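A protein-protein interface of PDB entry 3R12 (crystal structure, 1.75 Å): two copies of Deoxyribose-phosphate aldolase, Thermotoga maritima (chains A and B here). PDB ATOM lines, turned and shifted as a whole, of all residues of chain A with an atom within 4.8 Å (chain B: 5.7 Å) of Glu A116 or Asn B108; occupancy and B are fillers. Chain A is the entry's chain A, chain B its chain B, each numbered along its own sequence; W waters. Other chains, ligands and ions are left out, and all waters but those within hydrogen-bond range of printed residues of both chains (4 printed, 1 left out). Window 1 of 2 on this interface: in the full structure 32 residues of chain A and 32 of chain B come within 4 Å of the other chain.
The side-chain sulfur (SG) of Cys A81 sits at hydrogen-bond distance from the side-chain amide nitrogen (ND2) of Asn B133, 3.5 Å away. The side-chain carboxylate of Glu A116 sits at hydrogen-bond distance from the side-chain amide nitrogen of Asn B108. The backbone carbonyl oxygen (O) of Ala B107 lies within hydrogen-bond range of the backbone NH (N) of Cys A81, at 2.8 Å. OE2 of Glu B109 lies close to O of Phe A119. N of Pro A80 lies close to O of Ala B107 (3.5 Å).
The backbone carbonyl oxygen of Gly B106 sits close to the side-chain amide nitrogen of Asn B133 (3.5 Å). N of Gly A102 sits at hydrogen-bond distance from OE1 of Glu A116, 2.9 Å away.
Among the printed residues, merely in contact across the chains: Phe A119 with Thr B112 (3.3 Å), Cys A81 with Tyr B144 (3.6 Å), Glu A116 with Thr B112 (3.7 Å), Pro A80 with Glu B109 (3.8 Å), Cys A81 with Asn B108 (3.8 Å), Ala A120 with Glu B109 (3.8 Å) and Cys A81 with Glu B109 (3.998 Å).
Glu A116 touches two residues of chain B. Of the printed residues of chain A, Asn B108 touches Cys A81 (3.8 Å) and Glu A116 (2.7 Å). Of the printed residues of chain A, Ala B107 touches Pro A80 (3.5 Å) and Cys A81 (2.8 Å). Of the printed residues of chain B, Cys A81 touches Ala B107 (2.8 Å), Asn B108 (3.8 Å), Glu B109 (3.998 Å), Asn B133 (3.5 Å) and Tyr B144 (3.6 Å). Of the printed residues of chain B, Ala A120 touches Glu B109 (3.8 Å). The nearest residue of chain A that does not touch Asn B108 is Pro A80 (4.1 Å). The nearest printed residue of chain A that does not touch Asn B133 is Pro A80 (7.3 Å).
Hydrophobic or aromatic side chains of chain A within 4 Å of the printed part of chain B: Pro A80 and Phe A119. Of the 14 printed residues of chain B, 6 touch a printed residue of chain A. Hydrophobic or aromatic side chains of chain B that line the printed part of chain A: Tyr B144. Among the printed residues, no Asp or Glu carboxylate lies within 4 Å of a Lys or Arg side-chain nitrogen of the other chain.
Positions printed for both chains: 101, 102, 112 and 113. Of the 12 pairs that touch across the chains among the printed residues, none has its exchanged pair printed and touching as well.
Water W3 lies within hydrogen-bond range of OE1 of Glu A116 (2.7 Å) and ND2 of Asn B108 (3.4 Å). Water W1 lies within hydrogen-bond range of the side-chain hydroxyl of Thr B112, the side-chain carboxylate of Glu A116 and the backbone NH of Glu B109. Water W4 lies within hydrogen-bond range of O of Val A100, OE1 of Glu A116, N of Gly A102 and ND2 of Asn B108. Water W2 lies within hydrogen-bond range of the backbone carbonyl oxygen of Glu A116 (2.9 Å), the side-chain carboxylate of Glu B109 (3.0 Å) and the backbone NH of Ala A120 (3.4 Å).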
ATOM      1  N   PRO A  80      17.455   7.310  27.352  1.00  0.00           N
ATOM      2  CA  PRO A  80      16.533   8.307  26.787  1.00  0.00           C
ATOM      3  C   PRO A  80      16.236   9.527  27.652  1.00  0.00           C
ATOM      4  O   PRO A  80      16.025  10.624  27.104  1.00  0.00           O
ATOM      5  CB  PRO A  80      15.245   7.493  26.545  1.00  0.00           C
ATOM      6  CG  PRO A  80      15.736   6.090  26.283  1.00  0.00           C
ATOM      7  CD  PRO A  80      16.952   5.932  27.200  1.00  0.00           C
ATOM      8  N   CYS A  81      16.210   9.357  28.975  1.00  0.00           N
ATOM      9  CA  CYS A  81      15.903  10.486  29.845  1.00  0.00           C
ATOM     10  C   CYS A  81      16.932  11.632  29.708  1.00  0.00           C
ATOM     11  O   CYS A  81      16.632  12.773  30.075  1.00  0.00           O
ATOM     12  CB  CYS A  81      15.818  10.043  31.302  1.00  0.00           C
ATOM     13  SG  CYS A  81      17.402   9.454  31.971  1.00  0.00           S
ATOM     14  N   VAL A 100      19.100   4.670  23.253  1.00  0.00           N
ATOM     15  CA  VAL A 100      18.755   3.269  23.194  1.00  0.00           C
ATOM     16  C   VAL A 100      17.239   3.088  23.345  1.00  0.00           C
ATOM     17  O   VAL A 100      16.559   3.846  24.070  1.00  0.00           O
ATOM     18  CB  VAL A 100      19.514   2.463  24.254  1.00  0.00           C
ATOM     19  CG1 VAL A 100      21.075   2.452  23.961  1.00  0.00           C
ATOM     20  CG2 VAL A 100      19.185   2.987  25.682  1.00  0.00           C
ATOM     21  N   VAL A 101      16.704   2.083  22.660  1.00  0.00           N
ATOM     22  CA  VAL A 101      15.251   1.837  22.591  1.00  0.00           C
ATOM     23  C   VAL A 101      15.019   0.392  22.958  1.00  0.00           C
ATOM     24  O   VAL A 101      15.670  -0.529  22.413  1.00  0.00           O
ATOM     25  CB  VAL A 101      14.677   2.127  21.182  1.00  0.00           C
ATOM     26  CG1 VAL A 101      13.363   1.423  20.929  1.00  0.00           C
ATOM     27  CG2 VAL A 101      14.562   3.641  20.960  1.00  0.00           C
ATOM     28  N   GLY A 102      14.096   0.188  23.886  1.00  0.00           N
ATOM     29  CA  GLY A 102      13.785  -1.151  24.396  1.00  0.00           C
ATOM     30  C   GLY A 102      14.977  -1.886  25.010  1.00  0.00           C
ATOM     31  O   GLY A 102      15.125  -3.128  24.884  1.00  0.00           O
ATOM     32  N   THR A 112       5.588   0.107  22.336  1.00  0.00           N
ATOM     33  CA  THR A 112       6.434   0.816  23.282  1.00  0.00           C
ATOM     34  C   THR A 112       7.756   1.184  22.668  1.00  0.00           C
ATOM     35  O   THR A 112       8.217   2.315  22.850  1.00  0.00           O
ATOM     36  CB  THR A 112       6.751  -0.018  24.569  1.00  0.00           C
ATOM     37  OG1 THR A 112       5.540  -0.430  25.198  1.00  0.00           O
ATOM     38  CG2 THR A 112       7.583   0.795  25.542  1.00  0.00           C
ATOM     39  N   LYS A 113       8.393   0.245  21.963  1.00  0.00           N
ATOM     40  CA  LYS A 113       9.665   0.543  21.312  1.00  0.00           C
ATOM     41  C   LYS A 113       9.475   1.672  20.278  1.00  0.00           C
ATOM     42  O   LYS A 113      10.283   2.616  20.183  1.00  0.00           O
ATOM     43  CB  LYS A 113      10.288  -0.690  20.630  1.00  0.00           C
ATOM     44  CG  LYS A 113      10.552  -1.890  21.545  1.00  0.00           C
ATOM     45  CD  LYS A 113      11.461  -2.961  20.923  1.00  0.00           C
ATOM     46  CE  LYS A 113      11.604  -4.211  21.820  1.00  0.00           C
ATOM     47  NZ  LYS A 113      12.369  -5.330  21.160  1.00  0.00           N
ATOM     48  N   ALA A 114       8.406   1.588  19.501  1.00  0.00           N
ATOM     49  CA  ALA A 114       8.145   2.579  18.456  1.00  0.00           C
ATOM     50  C   ALA A 114       7.898   3.980  19.052  1.00  0.00           C
ATOM     51  O   ALA A 114       8.485   4.987  18.581  1.00  0.00           O
ATOM     52  CB  ALA A 114       6.944   2.130  17.602  1.00  0.00           C
ATOM     53  N   HIS A 115       7.061   4.032  20.086  1.00  0.00           N
ATOM     54  CA  HIS A 115       6.823   5.261  20.843  1.00  0.00           C
ATOM     55  C   HIS A 115       8.112   5.815  21.434  1.00  0.00           C
ATOM     56  O   HIS A 115       8.357   7.009  21.327  1.00  0.00           O
ATOM     57  CB  HIS A 115       5.771   5.049  21.950  1.00  0.00           C
ATOM     58  CG  HIS A 115       4.360   5.121  21.447  1.00  0.00           C
ATOM     59  ND1 HIS A 115       3.796   4.131  20.678  1.00  0.00           N
ATOM     60  CD2 HIS A 115       3.419   6.084  21.563  1.00  0.00           C
ATOM     61  CE1 HIS A 115       2.559   4.469  20.355  1.00  0.00           C
ATOM     62  NE2 HIS A 115       2.309   5.655  20.881  1.00  0.00           N
ATOM     63  N   GLU A 116       8.930   4.952  22.060  1.00  0.00           N
ATOM     64  CA  GLU A 116      10.196   5.426  22.650  1.00  0.00           C
ATOM     65  C   GLU A 116      11.125   6.070  21.603  1.00  0.00           C
ATOM     66  O   GLU A 116      11.752   7.110  21.868  1.00  0.00           O
ATOM     67  CB  GLU A 116      10.902   4.294  23.405  1.00  0.00           C
ATOM     68  CG  GLU A 116      12.212   4.698  24.035  1.00  0.00           C
ATOM     69  CD  GLU A 116      12.658   3.735  25.118  1.00  0.00           C
ATOM     70  OE1 GLU A 116      12.713   2.509  24.825  1.00  0.00           O
ATOM     71  OE2 GLU A 116      12.933   4.201  26.262  1.00  0.00           O
ATOM     72  N   ALA A 117      11.199   5.453  20.418  1.00  0.00           N
ATOM     73  CA  ALA A 117      11.979   5.965  19.302  1.00  0.00           C
ATOM     74  C   ALA A 117      11.483   7.326  18.855  1.00  0.00           C
ATOM     75  O   ALA A 117      12.282   8.230  18.660  1.00  0.00           O
ATOM     76  CB  ALA A 117      11.970   4.953  18.103  1.00  0.00           C
ATOM     77  N   ILE A 118      10.162   7.470  18.700  1.00  0.00           N
ATOM     78  CA  ILE A 118       9.560   8.731  18.309  1.00  0.00           C
ATOM     79  C   ILE A 118       9.864   9.805  19.359  1.00  0.00           C
ATOM     80  O   ILE A 118      10.289  10.893  19.041  1.00  0.00           O
ATOM     81  CB  ILE A 118       8.012   8.591  18.131  1.00  0.00           C
ATOM     82  CG1 ILE A 118       7.687   7.736  16.887  1.00  0.00           C
ATOM     83  CG2 ILE A 118       7.329   9.968  18.078  1.00  0.00           C
ATOM     84  CD1 ILE A 118       6.194   7.317  16.753  1.00  0.00           C
ATOM     85  N   PHE A 119       9.620   9.485  20.614  1.00  0.00           N
ATOM     86  CA  PHE A 119       9.952  10.403  21.719  1.00  0.00           C
ATOM     87  C   PHE A 119      11.441  10.803  21.710  1.00  0.00           C
ATOM     88  O   PHE A 119      11.766  11.965  21.929  1.00  0.00           O
ATOM     89  CB  PHE A 119       9.563   9.784  23.069  1.00  0.00           C
ATOM     90  CG  PHE A 119       8.076   9.499  23.222  1.00  0.00           C
ATOM     91  CD1 PHE A 119       7.107  10.219  22.495  1.00  0.00           C
ATOM     92  CD2 PHE A 119       7.644   8.522  24.098  1.00  0.00           C
ATOM     93  CE1 PHE A 119       5.766   9.954  22.646  1.00  0.00           C
ATOM     94  CE2 PHE A 119       6.301   8.263  24.250  1.00  0.00           C
ATOM     95  CZ  PHE A 119       5.358   8.970  23.509  1.00  0.00           C
ATOM     96  N   ALA A 120      12.327   9.849  21.428  1.00  0.00           N
ATOM     97  CA  ALA A 120      13.771  10.092  21.472  1.00  0.00           C
ATOM     98  C   ALA A 120      14.141  11.127  20.405  1.00  0.00           C
ATOM     99  O   ALA A 120      14.889  12.066  20.669  1.00  0.00           O
ATOM    100  CB  ALA A 120      14.551   8.773  21.268  1.00  0.00           C
ATOM    101  N   VAL B 101       7.975  -2.045  34.043  1.00  0.00           N
ATOM    102  CA  VAL B 101       7.904  -0.790  33.318  1.00  0.00           C
ATOM    103  C   VAL B 101       9.221  -0.029  33.518  1.00  0.00           C
ATOM    104  O   VAL B 101       9.721   0.119  34.624  1.00  0.00           O
ATOM    105  CB  VAL B 101       6.690   0.047  33.753  1.00  0.00           C
ATOM    106  CG1 VAL B 101       6.911   1.552  33.445  1.00  0.00           C
ATOM    107  CG2 VAL B 101       5.368  -0.531  33.097  1.00  0.00           C
ATOM    108  N   GLY B 102       9.790   0.440  32.420  1.00  0.00           N
ATOM    109  CA  GLY B 102      11.075   1.156  32.463  1.00  0.00           C
ATOM    110  C   GLY B 102      12.177   0.289  33.009  1.00  0.00           C
ATOM    111  O   GLY B 102      13.092   0.773  33.667  1.00  0.00           O
ATOM    112  N   PHE B 103      12.110  -1.005  32.703  1.00  0.00           N
ATOM    113  CA  PHE B 103      12.879  -2.006  33.404  1.00  0.00           C
ATOM    114  C   PHE B 103      13.973  -2.610  32.516  1.00  0.00           C
ATOM    115  O   PHE B 103      13.729  -2.916  31.335  1.00  0.00           O
ATOM    116  CB  PHE B 103      11.899  -3.088  33.880  1.00  0.00           C
ATOM    117  CG  PHE B 103      12.540  -4.282  34.565  1.00  0.00           C
ATOM    118  CD1 PHE B 103      13.106  -5.315  33.813  1.00  0.00           C
ATOM    119  CD2 PHE B 103      12.494  -4.418  35.951  1.00  0.00           C
ATOM    120  CE1 PHE B 103      13.670  -6.420  34.402  1.00  0.00           C
ATOM    121  CE2 PHE B 103      13.043  -5.528  36.567  1.00  0.00           C
ATOM    122  CZ  PHE B 103      13.664  -6.541  35.783  1.00  0.00           C
ATOM    123  N   LEU B 105      16.585  -0.515  33.920  1.00  0.00           N
ATOM    124  CA  LEU B 105      17.506   0.594  34.138  1.00  0.00           C
ATOM    125  C   LEU B 105      16.844   1.886  34.633  1.00  0.00           C
ATOM    126  O   LEU B 105      17.534   2.723  35.218  1.00  0.00           O
ATOM    127  CB  LEU B 105      18.319   0.905  32.874  1.00  0.00           C
ATOM    128  CG  LEU B 105      19.198  -0.235  32.330  1.00  0.00           C
ATOM    129  CD1 LEU B 105      20.171   0.347  31.264  1.00  0.00           C
ATOM    130  CD2 LEU B 105      19.932  -0.943  33.469  1.00  0.00           C
ATOM    131  N   GLY B 106      15.531   2.030  34.389  1.00  0.00           N
ATOM    132  CA  GLY B 106      14.724   3.138  34.918  1.00  0.00           C
ATOM    133  C   GLY B 106      15.031   4.478  34.305  1.00  0.00           C
ATOM    134  O   GLY B 106      14.636   5.534  34.837  1.00  0.00           O
ATOM    135  N   ALA B 107      15.689   4.461  33.144  1.00  0.00           N
ATOM    136  CA  ALA B 107      16.299   5.698  32.565  1.00  0.00           C
ATOM    137  C   ALA B 107      15.599   6.166  31.280  1.00  0.00           C
ATOM    138  O   ALA B 107      16.136   6.974  30.524  1.00  0.00           O
ATOM    139  CB  ALA B 107      17.796   5.486  32.313  1.00  0.00           C
ATOM    140  N   ASN B 108      14.427   5.576  31.011  1.00  0.00           N
ATOM    141  CA  ASN B 108      13.512   6.062  29.963  1.00  0.00           C
ATOM    142  C   ASN B 108      12.891   7.411  30.286  1.00  0.00           C
ATOM    143  O   ASN B 108      12.808   7.803  31.443  1.00  0.00           O
ATOM    144  CB  ASN B 108      12.370   5.057  29.729  1.00  0.00           C
ATOM    145  CG  ASN B 108      12.838   3.612  29.830  1.00  0.00           C
ATOM    146  OD1 ASN B 108      12.984   3.090  30.935  1.00  0.00           O
ATOM    147  ND2 ASN B 108      13.176   2.992  28.684  1.00  0.00           N
ATOM    148  N   GLU B 109      12.418   8.122  29.261  1.00  0.00           N
ATOM    149  CA  GLU B 109      11.592   9.285  29.490  1.00  0.00           C
ATOM    150  C   GLU B 109      10.359   8.898  30.298  1.00  0.00           C
ATOM    151  O   GLU B 109       9.787   7.814  30.107  1.00  0.00           O
ATOM    152  CB  GLU B 109      11.145   9.889  28.173  1.00  0.00           C
ATOM    153  CG  GLU B 109      12.284  10.501  27.362  1.00  0.00           C
ATOM    154  CD  GLU B 109      11.748  11.242  26.135  1.00  0.00           C
ATOM    155  OE1 GLU B 109      10.737  11.917  26.302  1.00  0.00           O
ATOM    156  OE2 GLU B 109      12.314  11.148  25.014  1.00  0.00           O
ATOM    157  N   THR B 110       9.911   9.798  31.171  1.00  0.00           N
ATOM    158  CA  THR B 110       8.686   9.559  31.948  1.00  0.00           C
ATOM    159  C   THR B 110       7.508   9.178  31.028  1.00  0.00           C
ATOM    160  O   THR B 110       6.739   8.264  31.336  1.00  0.00           O
ATOM    161  CB  THR B 110       8.376  10.761  32.871  1.00  0.00           C
ATOM    162  OG1 THR B 110       9.464  10.911  33.800  1.00  0.00           O
ATOM    163  CG2 THR B 110       7.015  10.567  33.618  1.00  0.00           C
ATOM    164  N   THR B 112       7.517   7.588  28.179  1.00  0.00           N
ATOM    165  CA  THR B 112       7.675   6.211  27.757  1.00  0.00           C
ATOM    166  C   THR B 112       7.219   5.237  28.864  1.00  0.00           C
ATOM    167  O   THR B 112       6.459   4.292  28.609  1.00  0.00           O
ATOM    168  CB  THR B 112       9.132   5.943  27.383  1.00  0.00           C
ATOM    169  OG1 THR B 112       9.488   6.822  26.288  1.00  0.00           O
ATOM    170  CG2 THR B 112       9.340   4.471  27.034  1.00  0.00           C
ATOM    171  N   LYS B 113       7.640   5.497  30.097  1.00  0.00           N
ATOM    172  CA  LYS B 113       7.165   4.681  31.237  1.00  0.00           C
ATOM    173  C   LYS B 113       5.635   4.702  31.369  1.00  0.00           C
ATOM    174  O   LYS B 113       5.001   3.640  31.498  1.00  0.00           O
ATOM    175  CB  LYS B 113       7.814   5.097  32.569  1.00  0.00           C
ATOM    176  CG  LYS B 113       9.347   4.943  32.618  1.00  0.00           C
ATOM    177  CD  LYS B 113       9.881   5.193  34.049  1.00  0.00           C
ATOM    178  CE  LYS B 113      11.384   5.374  34.132  1.00  0.00           C
ATOM    179  NZ  LYS B 113      11.897   5.455  35.520  1.00  0.00           N
ATOM    180  N   ASN B 133      14.053   6.234  38.484  1.00  0.00           N
ATOM    181  CA  ASN B 133      15.234   6.828  37.874  1.00  0.00           C
ATOM    182  C   ASN B 133      16.288   7.006  38.970  1.00  0.00           C
ATOM    183  O   ASN B 133      16.301   8.008  39.731  1.00  0.00           O
ATOM    184  CB  ASN B 133      14.891   8.115  37.137  1.00  0.00           C
ATOM    185  CG  ASN B 133      15.993   8.550  36.187  1.00  0.00           C
ATOM    186  OD1 ASN B 133      17.157   8.605  36.577  1.00  0.00           O
ATOM    187  ND2 ASN B 133      15.637   8.867  34.946  1.00  0.00           N
ATOM    188  N   TYR B 144      11.712  15.580  39.832  1.00  0.00           N
ATOM    189  CA  TYR B 144      11.773  14.691  38.690  1.00  0.00           C
ATOM    190  C   TYR B 144      11.362  13.265  39.065  1.00  0.00           C
ATOM    191  O   TYR B 144      10.536  12.680  38.385  1.00  0.00           O
ATOM    192  CB  TYR B 144      13.166  14.667  38.050  1.00  0.00           C
ATOM    193  CG  TYR B 144      13.196  13.757  36.839  1.00  0.00           C
ATOM    194  CD1 TYR B 144      13.328  12.378  36.985  1.00  0.00           C
ATOM    195  CD2 TYR B 144      13.052  14.268  35.565  1.00  0.00           C
ATOM    196  CE1 TYR B 144      13.337  11.528  35.883  1.00  0.00           C
ATOM    197  CE2 TYR B 144      13.070  13.424  34.448  1.00  0.00           C
ATOM    198  CZ  TYR B 144      13.226  12.060  34.624  1.00  0.00           C
ATOM    199  OH  TYR B 144      13.236  11.225  33.544  1.00  0.00           O
ATOM    200  N   ASP B 148       7.965  11.194  37.876  1.00  0.00           N
ATOM    201  CA  ASP B 148       8.246  10.002  37.058  1.00  0.00           C
ATOM    202  C   ASP B 148       7.372   8.863  37.578  1.00  0.00           C
ATOM    203  O   ASP B 148       6.760   8.133  36.805  1.00  0.00           O
ATOM    204  CB  ASP B 148       9.772   9.725  37.125  1.00  0.00           C
ATOM    205  CG  ASP B 148      10.237   8.555  36.260  1.00  0.00           C
ATOM    206  OD1 ASP B 148      10.213   8.675  35.020  1.00  0.00           O
ATOM    207  OD2 ASP B 148      10.652   7.523  36.832  1.00  0.00           O
HETATM  208  O   HOH W   1      12.193   6.840  26.641  1.00  0.00           O
HETATM  209  O   HOH W   2      12.554   8.221  24.450  1.00  0.00           O
HETATM  210  O   HOH W   3      11.925   0.634  26.620  1.00  0.00           O
HETATM  211  O   HOH W   4      15.528   2.203  26.225  1.00  0.00           O
